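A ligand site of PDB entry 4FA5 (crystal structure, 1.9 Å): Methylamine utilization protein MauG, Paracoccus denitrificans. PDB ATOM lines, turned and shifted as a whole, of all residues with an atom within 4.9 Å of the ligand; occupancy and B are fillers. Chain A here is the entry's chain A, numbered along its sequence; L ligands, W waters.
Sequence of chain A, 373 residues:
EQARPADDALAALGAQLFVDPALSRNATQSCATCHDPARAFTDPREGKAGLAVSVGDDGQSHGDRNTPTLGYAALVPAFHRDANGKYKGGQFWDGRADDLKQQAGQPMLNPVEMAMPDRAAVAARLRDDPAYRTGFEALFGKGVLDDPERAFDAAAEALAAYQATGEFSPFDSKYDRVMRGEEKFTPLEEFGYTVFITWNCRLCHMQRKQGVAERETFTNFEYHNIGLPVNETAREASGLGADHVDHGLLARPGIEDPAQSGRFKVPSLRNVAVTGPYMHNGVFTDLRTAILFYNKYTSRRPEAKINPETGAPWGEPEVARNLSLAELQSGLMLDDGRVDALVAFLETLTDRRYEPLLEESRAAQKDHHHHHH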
ATOM      1  N   PHE A  18      -8.866 -27.911  23.274  1.00  0.00           N
ATOM      2  CA  PHE A  18      -8.986 -27.018  22.169  1.00  0.00           C
ATOM      3  C   PHE A  18      -9.180 -25.608  22.694  1.00  0.00           C
ATOM      4  O   PHE A  18      -8.692 -24.644  22.073  1.00  0.00           O
ATOM      5  CB  PHE A  18     -10.183 -27.402  21.335  1.00  0.00           C
ATOM      6  CG  PHE A  18     -10.330 -26.578  20.094  1.00  0.00           C
ATOM      7  CD1 PHE A  18      -9.680 -26.971  18.930  1.00  0.00           C
ATOM      8  CD2 PHE A  18     -11.178 -25.443  20.078  1.00  0.00           C
ATOM      9  CE1 PHE A  18      -9.809 -26.245  17.742  1.00  0.00           C
ATOM     10  CE2 PHE A  18     -11.310 -24.695  18.912  1.00  0.00           C
ATOM     11  CZ  PHE A  18     -10.626 -25.103  17.738  1.00  0.00           C
ATOM     12  N   GLN A  29      -3.191 -18.241  25.320  1.00  0.00           N
ATOM     13  CA  GLN A  29      -3.712 -18.562  23.989  1.00  0.00           C
ATOM     14  C   GLN A  29      -4.158 -20.019  23.854  1.00  0.00           C
ATOM     15  O   GLN A  29      -3.408 -20.913  24.224  1.00  0.00           O
ATOM     16  CB  GLN A  29      -2.616 -18.263  22.975  1.00  0.00           C
ATOM     17  CG  GLN A  29      -3.056 -18.470  21.546  1.00  0.00           C
ATOM     18  CD  GLN A  29      -2.262 -17.631  20.588  1.00  0.00           C
ATOM     19  OE1 GLN A  29      -2.628 -16.455  20.286  1.00  0.00           O
ATOM     20  NE2 GLN A  29      -1.188 -18.215  20.072  1.00  0.00           N
ATOM     21  N   SER A  30      -5.368 -20.272  23.320  1.00  0.00           N
ATOM     22  CA  SER A  30      -5.718 -21.650  23.004  1.00  0.00           C
ATOM     23  C   SER A  30      -5.916 -21.799  21.499  1.00  0.00           C
ATOM     24  O   SER A  30      -5.961 -20.785  20.828  1.00  0.00           O
ATOM     25  CB  SER A  30      -6.984 -22.053  23.751  1.00  0.00           C
ATOM     26  OG  SER A  30      -8.109 -21.373  23.249  1.00  0.00           O
ATOM     27  N   CYS A  31      -6.066 -23.033  20.981  1.00  0.00           N
ATOM     28  CA  CYS A  31      -6.524 -23.192  19.544  1.00  0.00           C
ATOM     29  C   CYS A  31      -7.699 -22.270  19.258  1.00  0.00           C
ATOM     30  O   CYS A  31      -7.756 -21.657  18.186  1.00  0.00           O
ATOM     31  CB  CYS A  31      -7.035 -24.600  19.259  1.00  0.00           C
ATOM     32  SG  CYS A  31      -5.960 -25.922  19.733  1.00  0.00           S
ATOM     33  N   CYS A  34      -7.460 -18.483  18.097  1.00  0.00           N
ATOM     34  CA  CYS A  34      -7.323 -18.158  16.692  1.00  0.00           C
ATOM     35  C   CYS A  34      -8.384 -18.800  15.856  1.00  0.00           C
ATOM     36  O   CYS A  34      -8.798 -18.244  14.814  1.00  0.00           O
ATOM     37  CB  CYS A  34      -5.986 -18.615  16.186  1.00  0.00           C
ATOM     38  SG  CYS A  34      -4.593 -17.644  16.850  1.00  0.00           S
ATOM     39  N   HIS A  35      -8.819 -19.992  16.272  1.00  0.00           N
ATOM     40  CA  HIS A  35      -9.894 -20.646  15.534  1.00  0.00           C
ATOM     41  C   HIS A  35     -11.123 -20.549  16.380  1.00  0.00           C
ATOM     42  O   HIS A  35     -11.558 -21.506  17.034  1.00  0.00           O
ATOM     43  CB  HIS A  35      -9.553 -22.082  15.255  1.00  0.00           C
ATOM     44  CG  HIS A  35      -8.323 -22.261  14.434  1.00  0.00           C
ATOM     45  ND1 HIS A  35      -8.303 -22.093  13.052  1.00  0.00           N
ATOM     46  CD2 HIS A  35      -7.070 -22.609  14.785  1.00  0.00           C
ATOM     47  CE1 HIS A  35      -7.092 -22.372  12.604  1.00  0.00           C
ATOM     48  NE2 HIS A  35      -6.334 -22.703  13.637  1.00  0.00           N
ATOM     49  N   ARG A  45      -9.697 -11.534  15.952  1.00  0.00           N
ATOM     50  CA  ARG A  45      -8.825 -10.520  16.616  1.00  0.00           C
ATOM     51  C   ARG A  45      -8.090  -9.623  15.650  1.00  0.00           C
ATOM     52  O   ARG A  45      -7.338 -10.072  14.788  1.00  0.00           O
ATOM     53  CB  ARG A  45      -7.846 -11.114  17.640  1.00  0.00           C
ATOM     54  CG  ARG A  45      -8.463 -11.762  18.861  1.00  0.00           C
ATOM     55  CD  ARG A  45      -7.441 -12.600  19.628  1.00  0.00           C
ATOM     56  NE  ARG A  45      -6.650 -13.385  18.663  1.00  0.00           N
ATOM     57  CZ  ARG A  45      -5.378 -13.737  18.835  1.00  0.00           C
ATOM     58  NH1 ARG A  45      -4.713 -13.413  19.972  1.00  0.00           N
ATOM     59  NH2 ARG A  45      -4.788 -14.423  17.858  1.00  0.00           N
ATOM     60  N   SER A  54      -2.701 -13.692  12.223  1.00  0.00           N
ATOM     61  CA  SER A  54      -2.984 -13.801  13.647  1.00  0.00           C
ATOM     62  C   SER A  54      -1.768 -13.514  14.535  1.00  0.00           C
ATOM     63  O   SER A  54      -0.612 -13.685  14.092  1.00  0.00           O
ATOM     64  CB  SER A  54      -3.523 -15.205  13.913  1.00  0.00           C
ATOM     65  OG  SER A  54      -4.837 -15.345  13.383  1.00  0.00           O
ATOM     66  N   VAL A  55      -2.028 -13.119  15.787  1.00  0.00           N
ATOM     67  CA  VAL A  55      -0.981 -12.858  16.775  1.00  0.00           C
ATOM     68  C   VAL A  55      -0.854 -13.977  17.774  1.00  0.00           C
ATOM     69  O   VAL A  55      -1.867 -14.473  18.295  1.00  0.00           O
ATOM     70  CB  VAL A  55      -1.241 -11.522  17.493  1.00  0.00           C
ATOM     71  CG1 VAL A  55      -0.078 -11.141  18.455  1.00  0.00           C
ATOM     72  CG2 VAL A  55      -1.454 -10.431  16.458  1.00  0.00           C
ATOM     73  N   GLY A  56       0.381 -14.413  18.008  1.00  0.00           N
ATOM     74  CA  GLY A  56       0.628 -15.490  18.955  1.00  0.00           C
ATOM     75  C   GLY A  56       0.517 -15.121  20.442  1.00  0.00           C
ATOM     76  O   GLY A  56       0.234 -13.973  20.853  1.00  0.00           O
ATOM     77  N   ARG A  65       0.414 -15.920   7.252  1.00  0.00           N
ATOM     78  CA  ARG A  65      -0.747 -16.501   6.586  1.00  0.00           C
ATOM     79  C   ARG A  65      -2.026 -16.315   7.376  1.00  0.00           C
ATOM     80  O   ARG A  65      -2.026 -16.206   8.608  1.00  0.00           O
ATOM     81  CB  ARG A  65      -0.545 -17.999   6.306  1.00  0.00           C
ATOM     82  CG  ARG A  65       0.641 -18.284   5.395  1.00  0.00           C
ATOM     83  CD  ARG A  65       0.665 -19.696   4.943  1.00  0.00           C
ATOM     84  NE  ARG A  65       1.705 -19.936   3.908  1.00  0.00           N
ATOM     85  CZ  ARG A  65       2.430 -21.049   3.819  1.00  0.00           C
ATOM     86  NH1 ARG A  65       2.238 -22.030   4.683  1.00  0.00           N
ATOM     87  NH2 ARG A  65       3.312 -21.213   2.843  1.00  0.00           N
ATOM     88  N   ASN A  66      -3.127 -16.291   6.636  1.00  0.00           N
ATOM     89  CA  ASN A  66      -4.441 -16.059   7.237  1.00  0.00           C
ATOM     90  C   ASN A  66      -4.868 -17.342   7.928  1.00  0.00           C
ATOM     91  O   ASN A  66      -4.666 -18.476   7.393  1.00  0.00           O
ATOM     92  CB  ASN A  66      -5.420 -15.685   6.137  1.00  0.00           C
ATOM     93  CG  ASN A  66      -6.830 -15.472   6.631  1.00  0.00           C
ATOM     94  OD1 ASN A  66      -7.773 -16.186   6.156  1.00  0.00           O
ATOM     95  ND2 ASN A  66      -7.018 -14.453   7.540  1.00  0.00           N
ATOM     96  N   THR A  67      -5.383 -17.198   9.150  1.00  0.00           N
ATOM     97  CA  THR A  67      -5.889 -18.352   9.837  1.00  0.00           C
ATOM     98  C   THR A  67      -7.123 -18.942   9.127  1.00  0.00           C
ATOM     99  O   THR A  67      -8.137 -18.269   9.010  1.00  0.00           O
ATOM    100  CB  THR A  67      -6.233 -17.959  11.265  1.00  0.00           C
ATOM    101  OG1 THR A  67      -5.029 -17.563  11.929  1.00  0.00           O
ATOM    102  CG2 THR A  67      -6.894 -19.151  11.972  1.00  0.00           C
ATOM    103  N   PRO A  68      -7.036 -20.183   8.640  1.00  0.00           N
ATOM    104  CA  PRO A  68      -8.172 -20.784   7.974  1.00  0.00           C
ATOM    105  C   PRO A  68      -9.177 -21.403   8.978  1.00  0.00           C
ATOM    106  O   PRO A  68      -8.812 -21.851  10.096  1.00  0.00           O
ATOM    107  CB  PRO A  68      -7.522 -21.932   7.117  1.00  0.00           C
ATOM    108  CG  PRO A  68      -6.372 -22.353   7.940  1.00  0.00           C
ATOM    109  CD  PRO A  68      -5.907 -21.138   8.761  1.00  0.00           C
ATOM    110  N   THR A  69     -10.419 -21.539   8.542  1.00  0.00           N
ATOM    111  CA  THR A  69     -11.394 -22.372   9.241  1.00  0.00           C
ATOM    112  C   THR A  69     -10.907 -23.810   9.450  1.00  0.00           C
ATOM    113  O   THR A  69     -10.236 -24.416   8.603  1.00  0.00           O
ATOM    114  CB  THR A  69     -12.702 -22.393   8.489  1.00  0.00           C
ATOM    115  OG1 THR A  69     -13.688 -23.049   9.281  1.00  0.00           O
ATOM    116  CG2 THR A  69     -12.526 -23.152   7.107  1.00  0.00           C
ATOM    117  N   LEU A  70     -11.327 -24.377  10.554  1.00  0.00           N
ATOM    118  CA  LEU A  70     -11.210 -25.775  10.809  1.00  0.00           C
ATOM    119  C   LEU A  70     -12.475 -26.523  10.348  1.00  0.00           C
ATOM    120  O   LEU A  70     -12.484 -27.752  10.329  1.00  0.00           O
ATOM    121  CB  LEU A  70     -10.982 -26.020  12.317  1.00  0.00           C
ATOM    122  CG  LEU A  70      -9.725 -25.266  12.819  1.00  0.00           C
ATOM    123  CD1 LEU A  70      -9.408 -25.630  14.292  1.00  0.00           C
ATOM    124  CD2 LEU A  70      -8.494 -25.572  11.938  1.00  0.00           C
ATOM    125  N   ALA A  73     -12.260 -29.406   7.569  1.00  0.00           N
ATOM    126  CA  ALA A  73     -10.877 -29.740   7.295  1.00  0.00           C
ATOM    127  C   ALA A  73     -10.731 -31.235   7.495  1.00  0.00           C
ATOM    128  O   ALA A  73      -9.872 -31.877   6.904  1.00  0.00           O
ATOM    129  CB  ALA A  73      -9.929 -28.958   8.167  1.00  0.00           C
ATOM    130  N   GLN A  91      -2.712 -30.532   5.212  1.00  0.00           N
ATOM    131  CA  GLN A  91      -3.241 -29.401   6.013  1.00  0.00           C
ATOM    132  C   GLN A  91      -2.213 -28.295   5.999  1.00  0.00           C
ATOM    133  O   GLN A  91      -1.013 -28.566   5.761  1.00  0.00           O
ATOM    134  CB  GLN A  91      -3.490 -29.786   7.500  1.00  0.00           C
ATOM    135  CG  GLN A  91      -4.515 -30.921   7.673  1.00  0.00           C
ATOM    136  CD  GLN A  91      -5.932 -30.565   7.255  1.00  0.00           C
ATOM    137  OE1 GLN A  91      -6.735 -31.469   6.913  1.00  0.00           O
ATOM    138  NE2 GLN A  91      -6.264 -29.302   7.301  1.00  0.00           N
ATOM    139  N   PHE A  92      -2.719 -27.092   6.304  1.00  0.00           N
ATOM    140  CA  PHE A  92      -2.021 -25.806   6.127  1.00  0.00           C
ATOM    141  C   PHE A  92      -2.156 -25.411   4.644  1.00  0.00           C
ATOM    142  O   PHE A  92      -2.380 -26.239   3.751  1.00  0.00           O
ATOM    143  CB  PHE A  92      -0.529 -25.853   6.471  1.00  0.00           C
ATOM    144  CG  PHE A  92      -0.220 -26.010   7.919  1.00  0.00           C
ATOM    145  CD1 PHE A  92      -0.677 -25.076   8.859  1.00  0.00           C
ATOM    146  CD2 PHE A  92       0.660 -27.026   8.336  1.00  0.00           C
ATOM    147  CE1 PHE A  92      -0.335 -25.161  10.233  1.00  0.00           C
ATOM    148  CE2 PHE A  92       0.988 -27.143   9.697  1.00  0.00           C
ATOM    149  CZ  PHE A  92       0.512 -26.197  10.637  1.00  0.00           C
ATOM    150  N   TRP A  93      -1.972 -24.156   4.372  1.00  0.00           N
ATOM    151  CA  TRP A  93      -2.135 -23.655   3.016  1.00  0.00           C
ATOM    152  C   TRP A  93      -1.141 -24.233   2.045  1.00  0.00           C
ATOM    153  O   TRP A  93      -1.381 -24.279   0.827  1.00  0.00           O
ATOM    154  CB  TRP A  93      -1.963 -22.165   3.101  1.00  0.00           C
ATOM    155  CG  TRP A  93      -3.079 -21.411   3.709  1.00  0.00           C
ATOM    156  CD1 TRP A  93      -3.131 -20.876   4.969  1.00  0.00           C
ATOM    157  CD2 TRP A  93      -4.273 -21.001   3.053  1.00  0.00           C
ATOM    158  NE1 TRP A  93      -4.283 -20.172   5.130  1.00  0.00           N
ATOM    159  CE2 TRP A  93      -5.003 -20.212   3.971  1.00  0.00           C
ATOM    160  CE3 TRP A  93      -4.783 -21.187   1.742  1.00  0.00           C
ATOM    161  CZ2 TRP A  93      -6.237 -19.630   3.647  1.00  0.00           C
ATOM    162  CZ3 TRP A  93      -6.044 -20.623   1.436  1.00  0.00           C
ATOM    163  CH2 TRP A  93      -6.739 -19.835   2.365  1.00  0.00           C
ATOM    164  N   ASP A  94      -0.021 -24.718   2.591  1.00  0.00           N
ATOM    165  CA  ASP A  94       1.015 -25.312   1.782  1.00  0.00           C
ATOM    166  C   ASP A  94       1.101 -26.819   1.947  1.00  0.00           C
ATOM    167  O   ASP A  94       2.076 -27.410   1.546  1.00  0.00           O
ATOM    168  CB  ASP A  94       2.358 -24.624   2.042  1.00  0.00           C
ATOM    169  CG  ASP A  94       2.791 -24.715   3.489  1.00  0.00           C
ATOM    170  OD1 ASP A  94       3.777 -24.018   3.865  1.00  0.00           O
ATOM    171  OD2 ASP A  94       2.123 -25.446   4.270  1.00  0.00           O
ATOM    172  N   ARG A  96       1.967 -28.699   4.118  1.00  0.00           N
ATOM    173  CA  ARG A  96       3.143 -29.248   4.743  1.00  0.00           C
ATOM    174  C   ARG A  96       2.820 -30.252   5.900  1.00  0.00           C
ATOM    175  O   ARG A  96       3.689 -31.015   6.295  1.00  0.00           O
ATOM    176  CB  ARG A  96       4.059 -28.102   5.187  1.00  0.00           C
ATOM    177  CG  ARG A  96       3.545 -27.345   6.404  1.00  0.00           C
ATOM    178  CD  ARG A  96       4.553 -26.213   6.841  1.00  0.00           C
ATOM    179  NE  ARG A  96       4.089 -25.495   8.047  1.00  0.00           N
ATOM    180  CZ  ARG A  96       3.165 -24.524   8.026  1.00  0.00           C
ATOM    181  NH1 ARG A  96       2.787 -23.938   9.156  1.00  0.00           N
ATOM    182  NH2 ARG A  96       2.607 -24.159   6.884  1.00  0.00           N
ATOM    183  N   LEU A 100      -4.691 -34.014   9.961  1.00  0.00           N
ATOM    184  CA  LEU A 100      -4.973 -33.196  11.181  1.00  0.00           C
ATOM    185  C   LEU A 100      -4.110 -33.588  12.386  1.00  0.00           C
ATOM    186  O   LEU A 100      -3.716 -32.732  13.168  1.00  0.00           O
ATOM    187  CB  LEU A 100      -6.429 -33.338  11.598  1.00  0.00           C
ATOM    188  CG  LEU A 100      -7.379 -32.680  10.610  1.00  0.00           C
ATOM    189  CD1 LEU A 100      -8.813 -33.268  10.805  1.00  0.00           C
ATOM    190  CD2 LEU A 100      -7.296 -31.071  10.740  1.00  0.00           C
ATOM    191  N   GLN A 103      -0.816 -32.054  12.001  1.00  0.00           N
ATOM    192  CA  GLN A 103      -0.898 -30.591  12.083  1.00  0.00           C
ATOM    193  C   GLN A 103      -1.030 -30.093  13.578  1.00  0.00           C
ATOM    194  O   GLN A 103      -0.508 -29.056  13.918  1.00  0.00           O
ATOM    195  CB  GLN A 103      -2.123 -30.123  11.260  1.00  0.00           C
ATOM    196  CG  GLN A 103      -2.212 -28.595  11.115  1.00  0.00           C
ATOM    197  CD  GLN A 103      -2.547 -27.896  12.436  1.00  0.00           C
ATOM    198  OE1 GLN A 103      -3.178 -28.490  13.308  1.00  0.00           O
ATOM    199  NE2 GLN A 103      -2.127 -26.644  12.575  1.00  0.00           N
ATOM    200  N   ALA A 104      -1.687 -30.855  14.448  1.00  0.00           N
ATOM    201  CA  ALA A 104      -2.216 -30.334  15.746  1.00  0.00           C
ATOM    202  C   ALA A 104      -1.149 -29.871  16.690  1.00  0.00           C
ATOM    203  O   ALA A 104      -1.359 -28.929  17.452  1.00  0.00           O
ATOM    204  CB  ALA A 104      -3.192 -31.383  16.500  1.00  0.00           C
ATOM    205  N   PRO A 107       0.986 -25.735  16.021  1.00  0.00           N
ATOM    206  CA  PRO A 107       0.761 -24.435  16.717  1.00  0.00           C
ATOM    207  C   PRO A 107       1.321 -24.366  18.152  1.00  0.00           C
ATOM    208  O   PRO A 107       1.743 -23.279  18.611  1.00  0.00           O
ATOM    209  CB  PRO A 107      -0.773 -24.363  16.805  1.00  0.00           C
ATOM    210  CG  PRO A 107      -1.291 -25.307  15.780  1.00  0.00           C
ATOM    211  CD  PRO A 107      -0.268 -26.321  15.501  1.00  0.00           C
ATOM    212  N   MET A 108       1.245 -25.481  18.891  1.00  0.00           N
ATOM    213  CA  MET A 108       1.693 -25.548  20.271  1.00  0.00           C
ATOM    214  C   MET A 108       3.124 -25.168  20.482  1.00  0.00           C
ATOM    215  O   MET A 108       3.461 -24.642  21.529  1.00  0.00           O
ATOM    216  CB  MET A 108       1.505 -26.938  20.864  1.00  0.00           C
ATOM    217  CG  MET A 108       0.042 -27.294  20.984  1.00  0.00           C
ATOM    218  SD  MET A 108      -0.195 -28.897  21.741  1.00  0.00           S
ATOM    219  CE  MET A 108      -1.645 -29.495  20.881  1.00  0.00           C
ATOM    220  N   VAL A 112       5.890 -18.342  17.035  1.00  0.00           N
ATOM    221  CA  VAL A 112       5.020 -17.258  16.553  1.00  0.00           C
ATOM    222  C   VAL A 112       3.523 -17.457  16.904  1.00  0.00           C
ATOM    223  O   VAL A 112       2.726 -16.519  16.745  1.00  0.00           O
ATOM    224  CB  VAL A 112       5.266 -16.860  15.017  1.00  0.00           C
ATOM    225  CG1 VAL A 112       5.934 -17.954  14.255  1.00  0.00           C
ATOM    226  CG2 VAL A 112       4.020 -16.433  14.300  1.00  0.00           C
ATOM    227  N   GLU A 113       3.176 -18.636  17.435  1.00  0.00           N
ATOM    228  CA  GLU A 113       1.818 -18.976  17.852  1.00  0.00           C
ATOM    229  C   GLU A 113       1.781 -19.266  19.345  1.00  0.00           C
ATOM    230  O   GLU A 113       2.052 -18.371  20.174  1.00  0.00           O
ATOM    231  CB  GLU A 113       1.193 -20.109  16.949  1.00  0.00           C
ATOM    232  CG  GLU A 113       1.132 -19.622  15.466  1.00  0.00           C
ATOM    233  CD  GLU A 113       0.730 -20.718  14.446  1.00  0.00           C
ATOM    234  OE1 GLU A 113       0.815 -21.905  14.805  1.00  0.00           O
ATOM    235  OE2 GLU A 113       0.315 -20.393  13.297  1.00  0.00           O
ATOM    236  N   MET A 114       1.486 -20.488  19.715  1.00  0.00           N
ATOM    237  CA  MET A 114       1.311 -20.788  21.110  1.00  0.00           C
ATOM    238  C   MET A 114       2.634 -20.794  21.881  1.00  0.00           C
ATOM    239  O   MET A 114       2.651 -20.555  23.084  1.00  0.00           O
ATOM    240  CB  MET A 114       0.461 -22.039  21.303  1.00  0.00           C
ATOM    241  CG  MET A 114      -0.912 -21.892  20.641  1.00  0.00           C
ATOM    242  SD  MET A 114      -1.891 -23.385  20.519  1.00  0.00           S
ATOM    243  CE  MET A 114      -2.326 -23.520  22.246  1.00  0.00           C
ATOM    244  N   LEU A 159      -7.191 -33.589  19.796  1.00  0.00           N
ATOM    245  CA  LEU A 159      -7.543 -32.450  18.929  1.00  0.00           C
ATOM    246  C   LEU A 159      -8.008 -32.884  17.502  1.00  0.00           C
ATOM    247  O   LEU A 159      -8.981 -32.332  16.967  1.00  0.00           O
ATOM    248  CB  LEU A 159      -6.358 -31.465  18.792  1.00  0.00           C
ATOM    249  CG  LEU A 159      -6.157 -30.778  20.136  1.00  0.00           C
ATOM    250  CD1 LEU A 159      -4.741 -30.225  20.239  1.00  0.00           C
ATOM    251  CD2 LEU A 159      -7.208 -29.638  20.382  1.00  0.00           C
ATOM    252  N   GLN A 163     -11.722 -32.389  15.898  1.00  0.00           N
ATOM    253  CA  GLN A 163     -11.990 -31.742  14.578  1.00  0.00           C
ATOM    254  C   GLN A 163     -12.741 -32.595  13.559  1.00  0.00           C
ATOM    255  O   GLN A 163     -13.276 -32.058  12.561  1.00  0.00           O
ATOM    256  CB  GLN A 163     -10.734 -31.184  13.931  1.00  0.00           C
ATOM    257  CG  GLN A 163     -10.145 -29.998  14.736  1.00  0.00           C
ATOM    258  CD  GLN A 163      -8.750 -29.812  14.310  1.00  0.00           C
ATOM    259  OE1 GLN A 163      -7.824 -30.440  14.837  1.00  0.00           O
ATOM    260  NE2 GLN A 163      -8.560 -28.945  13.327  1.00  0.00           N
ATOM    261  N   LYS A 265      -3.046 -24.890  -1.379  1.00  0.00           N
ATOM    262  CA  LYS A 265      -4.217 -25.768  -1.334  1.00  0.00           C
ATOM    263  C   LYS A 265      -5.466 -25.008  -1.666  1.00  0.00           C
ATOM    264  O   LYS A 265      -5.706 -23.910  -1.115  1.00  0.00           O
ATOM    265  CB  LYS A 265      -4.399 -26.368   0.080  1.00  0.00           C
ATOM    266  CG  LYS A 265      -5.506 -27.397   0.187  1.00  0.00           C
ATOM    267  CD  LYS A 265      -5.414 -28.235   1.495  1.00  0.00           C
ATOM    268  CE  LYS A 265      -5.229 -27.402   2.798  1.00  0.00           C
ATOM    269  NZ  LYS A 265      -6.353 -26.431   3.180  1.00  0.00           N
HETATM  270 FE1  LIG L   1      -4.297 -23.255  13.597  1.00  0.00          FE
HETATM  271  C1  LIG L   1      -3.910 -23.688  10.241  1.00  0.00           C
HETATM  272  C2  LIG L   1      -5.630 -26.394  13.853  1.00  0.00           C
HETATM  273  C3  LIG L   1      -3.859 -23.101  17.000  1.00  0.00           C
HETATM  274  C4  LIG L   1      -3.565 -19.979  13.315  1.00  0.00           C
HETATM  275  N1  LIG L   1      -4.738 -24.796  12.252  1.00  0.00           N
HETATM  276  C5  LIG L   1      -4.499 -24.824  10.936  1.00  0.00           C
HETATM  277  C6  LIG L   1      -4.978 -26.053  10.253  1.00  0.00           C
HETATM  278  C7  LIG L   1      -5.439 -26.831  11.280  1.00  0.00           C
HETATM  279  C8  LIG L   1      -5.264 -25.990  12.503  1.00  0.00           C
HETATM  280  C9  LIG L   1      -6.044 -28.214  11.224  1.00  0.00           C
HETATM  281  C10 LIG L   1      -4.924 -26.365   8.758  1.00  0.00           C
HETATM  282  C11 LIG L   1      -6.239 -25.811   8.207  1.00  0.00           C
HETATM  283  C12 LIG L   1      -6.233 -25.962   6.671  1.00  0.00           C
HETATM  284  O1  LIG L   1      -7.259 -25.978   6.012  1.00  0.00           O
HETATM  285  O2  LIG L   1      -5.172 -26.091   6.077  1.00  0.00           O
HETATM  286  N2  LIG L   1      -4.700 -24.515  15.174  1.00  0.00           N
HETATM  287  C13 LIG L   1      -5.180 -25.773  15.102  1.00  0.00           C
HETATM  288  C14 LIG L   1      -5.227 -26.461  16.405  1.00  0.00           C
HETATM  289  C15 LIG L   1      -4.754 -25.503  17.308  1.00  0.00           C
HETATM  290  C16 LIG L   1      -4.420 -24.354  16.473  1.00  0.00           C
HETATM  291  C17 LIG L   1      -5.771 -27.863  16.580  1.00  0.00           C
HETATM  292  C18 LIG L   1      -4.527 -25.631  18.814  1.00  0.00           C
HETATM  293  C19 LIG L   1      -3.431 -26.647  19.060  1.00  0.00           C
HETATM  294  N3  LIG L   1      -3.807 -21.754  14.932  1.00  0.00           N
HETATM  295  C20 LIG L   1      -3.733 -21.839  16.274  1.00  0.00           C
HETATM  296  C21 LIG L   1      -3.458 -20.548  16.972  1.00  0.00           C
HETATM  297  C22 LIG L   1      -3.346 -19.619  15.920  1.00  0.00           C
HETATM  298  C23 LIG L   1      -3.584 -20.453  14.695  1.00  0.00           C
HETATM  299  C24 LIG L   1      -3.317 -20.398  18.464  1.00  0.00           C
HETATM  300  C25 LIG L   1      -3.075 -18.123  15.920  1.00  0.00           C
HETATM  301  C26 LIG L   1      -1.967 -17.645  16.827  1.00  0.00           C
HETATM  302  N4  LIG L   1      -3.870 -22.014  12.010  1.00  0.00           N
HETATM  303  C27 LIG L   1      -3.397 -20.785  12.100  1.00  0.00           C
HETATM  304  C28 LIG L   1      -2.806 -20.281  10.838  1.00  0.00           C
HETATM  305  C29 LIG L   1      -2.872 -21.354   9.984  1.00  0.00           C
HETATM  306  C30 LIG L   1      -3.539 -22.378  10.794  1.00  0.00           C
HETATM  307  C31 LIG L   1      -2.168 -18.938  10.672  1.00  0.00           C
HETATM  308  C32 LIG L   1      -2.381 -21.468   8.553  1.00  0.00           C
HETATM  309  C33 LIG L   1      -0.865 -21.570   8.613  1.00  0.00           C
HETATM  310  C34 LIG L   1      -0.250 -22.037   7.312  1.00  0.00           C
HETATM  311  O3  LIG L   1       1.016 -22.066   7.296  1.00  0.00           O
HETATM  312  O4  LIG L   1      -0.971 -22.451   6.356  1.00  0.00           O
HETATM  313  O   HOH W   1      -0.903 -22.745  12.520  1.00  0.00           O
HETATM  314  O   HOH W   2      -9.773 -25.339   6.188  1.00  0.00           O
HETATM  315  O   HOH W   3      -5.692 -23.452   4.569  1.00  0.00           O
HETATM  316  O   HOH W   4      -1.217 -15.846  11.199  1.00  0.00           O
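A carbon (C18) of the ligand is covalently linked to the side-chain sulfur (SG) of Cys 31 (1.7 Å).
SG of Cys 34 is bonded to C25 of the ligand (1.8 Å).
A ring nitrogen (NE2) of His 35 is bound to an iron atom (FE1) of the ligand (2.1 Å).
An oxygen (O2) of the ligand is in hydrogen-bond range of the backbone NH of Phe 92, 2.7 Å away.
An oxygen (O3) of the ligand is in salt-bridge range of the guanidinium group of Arg 96.
N of Trp 93 lies within hydrogen-bond range of O4 of the ligand (2.8 Å).
The guanidinium group of Arg 65 lies within salt-bridge range of an oxygen (O3) of the ligand (2.9 Å).
An oxygen (O1) of the ligand lies within salt-bridge range of the side-chain amino group (NZ) of Lys 265, at 3.0 Å.
The backbone NH of Cys 31 lies close to the backbone carbonyl oxygen of Phe 18, 3.3 Å away.
SG of Cys 34 is in hydrogen-bond range of NH2 of Arg 45 (3.4 Å).
A ring nitrogen (ND1) of His 35 lies within hydrogen-bond range of the backbone carbonyl oxygen of Pro 68, 3.0 Å away.
The backbone carbonyl oxygen (O) of Gln 91 sits at hydrogen-bond distance from the backbone NH (N) of Arg 96.
The guanidinium group of Arg 96 is in salt-bridge range of the side-chain carboxylate of Asp 94, at 3.0 Å.
The backbone carbonyl oxygen (O) of Trp 93 sits at hydrogen-bond distance from the backbone NH (N) of Lys 265, at 2.8 Å.
The guanidinium group (NH1) of Arg 65 lies within salt-bridge range of the side-chain carboxylate (OD1) of Asp 94, at 2.6 Å.
The backbone carbonyl oxygen (O) of Val 112 sits close to the backbone NH (N) of Gly 56, 3.4 Å away.
N1 of the ligand lies close to NE2 of Gln 103, 3.2 Å away.
Residues that only touch the ligand: Gln 29 (3.4 Å), Ser 30 (3.6 Å), Ser 54 (3.6 Å), Val 55 (3.5 Å), Gly 56 (3.99 Å), Asn 66 (3.9 Å), Thr 67 (3.1 Å), Pro 68 (3.3 Å), Leu 70 (3.3 Å), Gln 91 (3.4 Å), Leu 100 (3.2 Å), Ala 104 (3.5 Å), Pro 107 (3.3 Å), Met 108 (3.8 Å), Glu 113 (3.9 Å), Met 114 (3.6 Å), Leu 159 (3.99 Å) and Gln 163 (3.4 Å).
Hydrophobic or aromatic side chains that line the ligand: His 35, Pro 68, Leu 70, Phe 92, Trp 93, Leu 100, Pro 107, Met 108, Met 114 and Leu 159.
27 residues have an atom within 4 Å of the ligand: Gln 29, Ser 30, Cys 31, Cys 34, His 35, Ser 54, Val 55, Gly 56, Arg 65, Asn 66, Thr 67, Pro 68, Leu 70, Gln 91, Phe 92, Trp 93, Arg 96, Leu 100, Gln 103, Ala 104, Pro 107, Met 108, Glu 113, Met 114, Leu 159, Gln 163 and Lys 265.
Water W2 lies within hydrogen-bond range of O1 of the ligand (2.6 Å) and O of Thr 69 (2.6 Å).
Water W3 lies within hydrogen-bond range of O2 of the ligand and NZ of Lys 265.
Water W4 lies within hydrogen-bond range of the backbone carbonyl oxygen of Arg 65 (2.7 Å) and the backbone NH of Ser 54 (2.8 Å).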
